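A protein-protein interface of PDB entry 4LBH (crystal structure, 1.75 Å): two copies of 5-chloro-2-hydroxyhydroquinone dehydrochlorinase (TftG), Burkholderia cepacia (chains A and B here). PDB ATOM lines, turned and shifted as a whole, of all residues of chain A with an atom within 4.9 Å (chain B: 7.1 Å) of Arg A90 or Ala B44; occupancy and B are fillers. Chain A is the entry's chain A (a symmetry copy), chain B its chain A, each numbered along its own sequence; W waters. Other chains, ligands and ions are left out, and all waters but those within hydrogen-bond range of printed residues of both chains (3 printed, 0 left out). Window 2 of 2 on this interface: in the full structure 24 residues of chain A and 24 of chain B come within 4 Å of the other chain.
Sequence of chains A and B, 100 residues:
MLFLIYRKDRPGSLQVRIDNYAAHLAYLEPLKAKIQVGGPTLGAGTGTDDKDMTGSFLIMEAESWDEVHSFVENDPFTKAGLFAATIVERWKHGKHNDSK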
ATOM      1  N   MET A   1     -13.263  23.619  20.501  1.00  0.00           N
ATOM      2  CA  MET A   1     -12.865  22.283  20.083  1.00  0.00           C
ATOM      3  C   MET A   1     -11.525  22.414  19.377  1.00  0.00           C
ATOM      4  O   MET A   1     -11.149  23.511  18.961  1.00  0.00           O
ATOM      5  CB  MET A   1     -13.891  21.699  19.105  1.00  0.00           C
ATOM      6  CG  MET A   1     -15.290  21.493  19.677  1.00  0.00           C
ATOM      7  SD  MET A   1     -16.483  21.090  18.377  1.00  0.00           S
ATOM      8  CE  MET A   1     -16.330  22.573  17.390  1.00  0.00           C
ATOM      9  N   LEU A   2     -10.819  21.298  19.232  1.00  0.00           N
ATOM     10  CA  LEU A   2      -9.566  21.285  18.485  1.00  0.00           C
ATOM     11  C   LEU A   2      -9.728  20.500  17.204  1.00  0.00           C
ATOM     12  O   LEU A   2     -10.456  19.501  17.162  1.00  0.00           O
ATOM     13  CB  LEU A   2      -8.457  20.652  19.318  1.00  0.00           C
ATOM     14  CG  LEU A   2      -8.049  21.372  20.601  1.00  0.00           C
ATOM     15  CD1 LEU A   2      -6.994  20.586  21.350  1.00  0.00           C
ATOM     16  CD2 LEU A   2      -7.555  22.771  20.287  1.00  0.00           C
ATOM     17  N   PHE A   3      -9.017  20.946  16.174  1.00  0.00           N
ATOM     18  CA  PHE A   3      -9.044  20.314  14.864  1.00  0.00           C
ATOM     19  C   PHE A   3      -7.632  20.114  14.336  1.00  0.00           C
ATOM     20  O   PHE A   3      -6.789  21.016  14.429  1.00  0.00           O
ATOM     21  CB  PHE A   3      -9.820  21.189  13.872  1.00  0.00           C
ATOM     22  CG  PHE A   3     -11.282  21.266  14.160  1.00  0.00           C
ATOM     23  CD1 PHE A   3     -12.157  20.347  13.598  1.00  0.00           C
ATOM     24  CD2 PHE A   3     -11.783  22.242  15.011  1.00  0.00           C
ATOM     25  CE1 PHE A   3     -13.515  20.415  13.862  1.00  0.00           C
ATOM     26  CE2 PHE A   3     -13.146  22.311  15.290  1.00  0.00           C
ATOM     27  CZ  PHE A   3     -14.008  21.400  14.713  1.00  0.00           C
ATOM     28  N   TRP A  65     -16.970  23.697  12.670  1.00  0.00           N
ATOM     29  CA  TRP A  65     -16.470  23.405  11.333  1.00  0.00           C
ATOM     30  C   TRP A  65     -16.564  24.629  10.414  1.00  0.00           C
ATOM     31  O   TRP A  65     -15.731  24.804   9.531  1.00  0.00           O
ATOM     32  CB  TRP A  65     -17.217  22.218  10.714  1.00  0.00           C
ATOM     33  CG  TRP A  65     -16.695  20.858  11.131  1.00  0.00           C
ATOM     34  CD1 TRP A  65     -17.055  20.137  12.242  1.00  0.00           C
ATOM     35  CD2 TRP A  65     -15.730  20.054  10.432  1.00  0.00           C
ATOM     36  NE1 TRP A  65     -16.367  18.940  12.276  1.00  0.00           N
ATOM     37  CE2 TRP A  65     -15.551  18.867  11.177  1.00  0.00           C
ATOM     38  CE3 TRP A  65     -14.999  20.225   9.252  1.00  0.00           C
ATOM     39  CZ2 TRP A  65     -14.672  17.856  10.776  1.00  0.00           C
ATOM     40  CZ3 TRP A  65     -14.133  19.219   8.854  1.00  0.00           C
ATOM     41  CH2 TRP A  65     -13.975  18.048   9.616  1.00  0.00           C
ATOM     42  N   VAL A  88      -9.235  17.303   7.425  1.00  0.00           N
ATOM     43  CA  VAL A  88      -9.569  17.961   8.686  1.00  0.00           C
ATOM     44  C   VAL A  88     -10.235  16.936   9.622  1.00  0.00           C
ATOM     45  O   VAL A  88     -11.070  16.160   9.174  1.00  0.00           O
ATOM     46  CB  VAL A  88     -10.496  19.166   8.449  1.00  0.00           C
ATOM     47  CG1 VAL A  88     -10.886  19.812   9.767  1.00  0.00           C
ATOM     48  CG2 VAL A  88      -9.806  20.194   7.522  1.00  0.00           C
ATOM     49  N   GLU A  89      -9.822  16.908  10.889  1.00  0.00           N
ATOM     50  CA  GLU A  89     -10.402  16.008  11.900  1.00  0.00           C
ATOM     51  C   GLU A  89     -10.572  16.724  13.222  1.00  0.00           C
ATOM     52  O   GLU A  89      -9.666  17.435  13.668  1.00  0.00           O
ATOM     53  CB  GLU A  89      -9.451  14.838  12.192  1.00  0.00           C
ATOM     54  CG  GLU A  89      -9.115  13.943  11.025  1.00  0.00           C
ATOM     55  CD  GLU A  89     -10.195  12.929  10.720  1.00  0.00           C
ATOM     56  OE1 GLU A  89     -11.220  12.893  11.436  1.00  0.00           O
ATOM     57  OE2 GLU A  89     -10.016  12.167   9.751  1.00  0.00           O
ATOM     58  N   ARG A  90     -11.707  16.511  13.882  1.00  0.00           N
ATOM     59  CA  ARG A  90     -11.832  16.961  15.258  1.00  0.00           C
ATOM     60  C   ARG A  90     -10.915  16.068  16.105  1.00  0.00           C
ATOM     61  O   ARG A  90     -10.671  14.902  15.763  1.00  0.00           O
ATOM     62  CB  ARG A  90     -13.295  16.884  15.717  1.00  0.00           C
ATOM     63  CG  ARG A  90     -13.549  17.539  17.057  1.00  0.00           C
ATOM     64  CD  ARG A  90     -15.048  17.658  17.328  1.00  0.00           C
ATOM     65  NE  ARG A  90     -15.737  16.382  17.548  1.00  0.00           N
ATOM     66  CZ  ARG A  90     -16.013  15.892  18.754  1.00  0.00           C
ATOM     67  NH1 ARG A  90     -15.621  16.554  19.841  1.00  0.00           N
ATOM     68  NH2 ARG A  90     -16.689  14.750  18.886  1.00  0.00           N
ATOM     69  N   TRP A  91     -10.365  16.607  17.191  1.00  0.00           N
ATOM     70  CA  TRP A  91      -9.305  15.897  17.907  1.00  0.00           C
ATOM     71  C   TRP A  91      -9.185  16.386  19.347  1.00  0.00           C
ATOM     72  O   TRP A  91      -9.592  17.501  19.655  1.00  0.00           O
ATOM     73  CB  TRP A  91      -7.967  16.101  17.152  1.00  0.00           C
ATOM     74  CG  TRP A  91      -6.727  15.487  17.794  1.00  0.00           C
ATOM     75  CD1 TRP A  91      -6.254  14.206  17.642  1.00  0.00           C
ATOM     76  CD2 TRP A  91      -5.782  16.160  18.641  1.00  0.00           C
ATOM     77  NE1 TRP A  91      -5.094  14.039  18.372  1.00  0.00           N
ATOM     78  CE2 TRP A  91      -4.780  15.225  18.980  1.00  0.00           C
ATOM     79  CE3 TRP A  91      -5.691  17.465  19.146  1.00  0.00           C
ATOM     80  CZ2 TRP A  91      -3.708  15.547  19.813  1.00  0.00           C
ATOM     81  CZ3 TRP A  91      -4.626  17.784  19.971  1.00  0.00           C
ATOM     82  CH2 TRP A  91      -3.648  16.828  20.295  1.00  0.00           C
ATOM     83  N   LYS A  92      -8.633  15.549  20.227  1.00  0.00           N
ATOM     84  CA  LYS A  92      -8.300  15.997  21.575  1.00  0.00           C
ATOM     85  C   LYS A  92      -7.001  15.361  22.051  1.00  0.00           C
ATOM     86  O   LYS A  92      -6.601  14.304  21.554  1.00  0.00           O
ATOM     87  CB  LYS A  92      -9.434  15.654  22.551  1.00  0.00           C
ATOM     88  CG  LYS A  92      -9.565  14.152  22.796  1.00  0.00           C
ATOM     89  CD  LYS A  92     -10.551  13.880  23.943  1.00  0.00           C
ATOM     90  CE  LYS A  92     -10.166  12.593  24.654  1.00  0.00           C
ATOM     91  NZ  LYS A  92     -11.094  12.213  25.765  1.00  0.00           N
ATOM     92  N   PRO B  40      -6.700  10.903  20.458  1.00  0.00           N
ATOM     93  CA  PRO B  40      -7.651  10.361  19.483  1.00  0.00           C
ATOM     94  C   PRO B  40      -8.280  11.442  18.606  1.00  0.00           C
ATOM     95  O   PRO B  40      -8.557  12.567  19.062  1.00  0.00           O
ATOM     96  CB  PRO B  40      -8.726   9.717  20.377  1.00  0.00           C
ATOM     97  CG  PRO B  40      -8.728  10.589  21.603  1.00  0.00           C
ATOM     98  CD  PRO B  40      -7.271  10.992  21.814  1.00  0.00           C
ATOM     99  N   THR B  41      -8.525  11.108  17.342  1.00  0.00           N
ATOM    100  CA  THR B  41      -9.448  11.906  16.558  1.00  0.00           C
ATOM    101  C   THR B  41     -10.869  11.588  17.049  1.00  0.00           C
ATOM    102  O   THR B  41     -11.129  10.519  17.622  1.00  0.00           O
ATOM    103  CB  THR B  41      -9.338  11.620  15.060  1.00  0.00           C
ATOM    104  OG1 THR B  41      -9.546  10.220  14.838  1.00  0.00           O
ATOM    105  CG2 THR B  41      -7.931  11.997  14.564  1.00  0.00           C
ATOM    106  N   LEU B  42     -11.768  12.540  16.831  1.00  0.00           N
ATOM    107  CA  LEU B  42     -13.124  12.464  17.371  1.00  0.00           C
ATOM    108  C   LEU B  42     -14.134  12.643  16.248  1.00  0.00           C
ATOM    109  O   LEU B  42     -13.853  13.290  15.235  1.00  0.00           O
ATOM    110  CB  LEU B  42     -13.319  13.562  18.417  1.00  0.00           C
ATOM    111  CG  LEU B  42     -12.349  13.509  19.605  1.00  0.00           C
ATOM    112  CD1 LEU B  42     -12.539  14.787  20.439  1.00  0.00           C
ATOM    113  CD2 LEU B  42     -12.535  12.260  20.479  1.00  0.00           C
ATOM    114  N   GLY B  43     -15.318  12.077  16.431  1.00  0.00           N
ATOM    115  CA  GLY B  43     -16.332  12.102  15.392  1.00  0.00           C
ATOM    116  C   GLY B  43     -17.341  13.228  15.522  1.00  0.00           C
ATOM    117  O   GLY B  43     -17.010  14.335  15.943  1.00  0.00           O
ATOM    118  N   ALA B  44     -18.585  12.940  15.152  1.00  0.00           N
ATOM    119  CA  ALA B  44     -19.638  13.961  15.139  1.00  0.00           C
ATOM    120  C   ALA B  44     -19.889  14.572  16.511  1.00  0.00           C
ATOM    121  O   ALA B  44     -19.658  13.933  17.539  1.00  0.00           O
ATOM    122  CB  ALA B  44     -20.926  13.372  14.591  1.00  0.00           C
ATOM    123  N   GLY B  45     -20.399  15.802  16.524  1.00  0.00           N
ATOM    124  CA  GLY B  45     -20.823  16.437  17.764  1.00  0.00           C
ATOM    125  C   GLY B  45     -19.688  17.049  18.559  1.00  0.00           C
ATOM    126  O   GLY B  45     -18.634  17.373  18.004  1.00  0.00           O
ATOM    127  N   THR B  46     -19.905  17.194  19.866  1.00  0.00           N
ATOM    128  CA  THR B  46     -18.951  17.858  20.750  1.00  0.00           C
ATOM    129  C   THR B  46     -18.442  16.948  21.863  1.00  0.00           C
ATOM    130  O   THR B  46     -17.668  17.389  22.712  1.00  0.00           O
ATOM    131  CB  THR B  46     -19.597  19.083  21.435  1.00  0.00           C
ATOM    132  OG1 THR B  46     -20.702  18.650  22.239  1.00  0.00           O
ATOM    133  CG2 THR B  46     -20.105  20.077  20.393  1.00  0.00           C
ATOM    134  N   GLY B  47     -18.868  15.689  21.863  1.00  0.00           N
ATOM    135  CA  GLY B  47     -18.490  14.773  22.930  1.00  0.00           C
ATOM    136  C   GLY B  47     -17.002  14.466  22.897  1.00  0.00           C
ATOM    137  O   GLY B  47     -16.394  14.422  21.824  1.00  0.00           O
ATOM    138  N   THR B  48     -16.411  14.264  24.071  1.00  0.00           N
ATOM    139  CA  THR B  48     -14.992  13.898  24.142  1.00  0.00           C
ATOM    140  C   THR B  48     -14.784  12.617  24.959  1.00  0.00           C
ATOM    141  O   THR B  48     -13.760  12.448  25.622  1.00  0.00           O
ATOM    142  CB  THR B  48     -14.157  15.038  24.751  1.00  0.00           C
ATOM    143  OG1 THR B  48     -14.717  15.401  26.021  1.00  0.00           O
ATOM    144  CG2 THR B  48     -14.167  16.271  23.821  1.00  0.00           C
ATOM    145  N   ASP B  49     -15.750  11.707  24.889  1.00  0.00           N
ATOM    146  CA  ASP B  49     -15.680  10.455  25.654  1.00  0.00           C
ATOM    147  C   ASP B  49     -15.093   9.334  24.808  1.00  0.00           C
ATOM    148  O   ASP B  49     -14.826   9.526  23.627  1.00  0.00           O
ATOM    149  CB  ASP B  49     -17.079  10.063  26.116  1.00  0.00           C
ATOM    150  CG  ASP B  49     -17.661  11.055  27.107  1.00  0.00           C
ATOM    151  OD1 ASP B  49     -16.941  11.461  28.045  1.00  0.00           O
ATOM    152  OD2 ASP B  49     -18.832  11.439  26.939  1.00  0.00           O
ATOM    153  N   ASP B  52     -16.614   8.615  21.426  1.00  0.00           N
ATOM    154  CA  ASP B  52     -16.403   9.616  20.376  1.00  0.00           C
ATOM    155  C   ASP B  52     -15.140   9.392  19.558  1.00  0.00           C
ATOM    156  O   ASP B  52     -14.931  10.082  18.556  1.00  0.00           O
ATOM    157  CB  ASP B  52     -16.357  11.003  21.006  1.00  0.00           C
ATOM    158  CG  ASP B  52     -17.684  11.386  21.619  1.00  0.00           C
ATOM    159  OD1 ASP B  52     -18.661  11.511  20.847  1.00  0.00           O
ATOM    160  OD2 ASP B  52     -17.760  11.520  22.865  1.00  0.00           O
ATOM    161  N   MET B  53     -14.305   8.443  19.980  1.00  0.00           N
ATOM    162  CA  MET B  53     -13.002   8.212  19.335  1.00  0.00           C
ATOM    163  C   MET B  53     -13.155   7.584  17.945  1.00  0.00           C
ATOM    164  O   MET B  53     -13.938   6.650  17.758  1.00  0.00           O
ATOM    165  CB  MET B  53     -12.110   7.308  20.218  1.00  0.00           C
ATOM    166  CG  MET B  53     -11.645   7.934  21.548  1.00  0.00           C
ATOM    167  SD  MET B  53     -10.379   6.993  22.471  1.00  0.00           S
ATOM    168  CE  MET B  53     -11.361   5.580  22.949  1.00  0.00           C
ATOM    169  N   THR B  54     -12.372   8.060  16.981  1.00  0.00           N
ATOM    170  CA  THR B  54     -12.479   7.562  15.617  1.00  0.00           C
ATOM    171  C   THR B  54     -11.121   7.234  14.979  1.00  0.00           C
ATOM    172  O   THR B  54     -11.072   6.796  13.831  1.00  0.00           O
ATOM    173  CB  THR B  54     -13.161   8.612  14.700  1.00  0.00           C
ATOM    174  OG1 THR B  54     -12.405   9.835  14.727  1.00  0.00           O
ATOM    175  CG2 THR B  54     -14.620   8.907  15.151  1.00  0.00           C
HETATM  176  O   HOH W   1     -13.321  11.568  12.935  1.00  0.00           O
HETATM  177  O   HOH W   2     -17.126  16.610  14.007  1.00  0.00           O
HETATM  178  O   HOH W   3     -13.914  14.941  12.930  1.00  0.00           O
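N of Lys A92 sits at hydrogen-bond distance from O of Pro B40, 3.2 Å away. N of Leu B42 lies within hydrogen-bond range of O of Arg A90 (2.8 Å). O of Gly B43 sits at hydrogen-bond distance from NE of Arg A90 (2.9 Å). The backbone carbonyl oxygen (O) of Ala B44 is in hydrogen-bond range of the guanidinium group (NH2) of Arg A90, at 3.4 Å. O of Gly B45 lies within hydrogen-bond range of NE of Arg A90, 3.1 Å away. O of Gly B47 lies within hydrogen-bond range of NH2 of Arg A90 (3.0 Å). O of Thr B48 is in hydrogen-bond range of NZ of Lys A92, 2.7 Å away.
The backbone carbonyl oxygen (O) of Thr B41 sits at hydrogen-bond distance from the backbone NH (N) of Thr B54 (2.8 Å). The backbone NH (N) of Leu B42 lies within hydrogen-bond range of the side-chain hydroxyl (OG1) of Thr B54 (3.5 Å). O of Asp B52 is in hydrogen-bond range of N of Gly B43 (2.9 Å). The backbone NH of Thr B48 lies within hydrogen-bond range of the side-chain carboxylate of Asp B52 (3.3 Å). The backbone carbonyl oxygen (O) of Leu A2 sits at hydrogen-bond distance from the backbone NH (N) of Trp A91 (2.9 Å).
CA of Thr B41 touches O of Arg A90, at 3.3 Å. C of Thr B46 touches NH1 of Arg A90, at 3.5 Å. O of Pro B40 touches CD1 of Trp A91 (3.2 Å). Thr B41 touches Trp A91. C of Trp A91 touches CD1 of Leu B42, 3.9 Å away. Lys A92 touches Leu B42 (CG to CD1, 3.8 Å).
Of chain B, only Thr B41 (3.3 Å), Leu B42 (2.8 Å), Gly B43 (2.9 Å), Ala B44 (3.4 Å), Gly B45 (3.1 Å), Thr B46 (3.5 Å) and Gly B47 (3.0 Å) come within 4 Å of Arg A90. Of the printed residues of chain B, Trp A91 touches Pro B40, Thr B41 and Leu B42. Of the printed residues of chain A, Thr B41 touches Arg A90 and Trp A91. Of chain A, only Arg A90 (3.4 Å) comes within 4 Å of Ala B44. Of the printed residues of chain A, Gly B45 touches Arg A90. Of the printed residues of chain A, Gly B47 touches Arg A90 (3.0 Å). Met B53 touches none of the printed residues of chain A. The nearest printed residue of chain A that does not touch Ala B44 is Trp A65 (6.6 Å).
Of the 13 printed residues of chain B, 9 touch a printed residue of chain A. Among the printed residues, 13 pairs touch across the chains. Among the printed residues, no Asp or Glu carboxylate lies within 4 Å of a Lys or Arg side-chain nitrogen of the other chain.
No position is printed for both chains. Of the 13 pairs that touch across the chains among the printed residues, none has its exchanged pair printed and touching as well.
Water W1 lies within hydrogen-bond range of OG1 of Thr B54 (2.7 Å), OE1 of Glu A89 (2.9 Å) and O of Leu B42 (2.9 Å). Water W3 bridges the backbone carbonyl oxygen (O) of Leu B42 (2.8 Å) and the backbone NH (N) of Arg A90 (2.9 Å). Water W2 lies within hydrogen-bond range of O of Gly B43 and NE1 of Trp A65.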
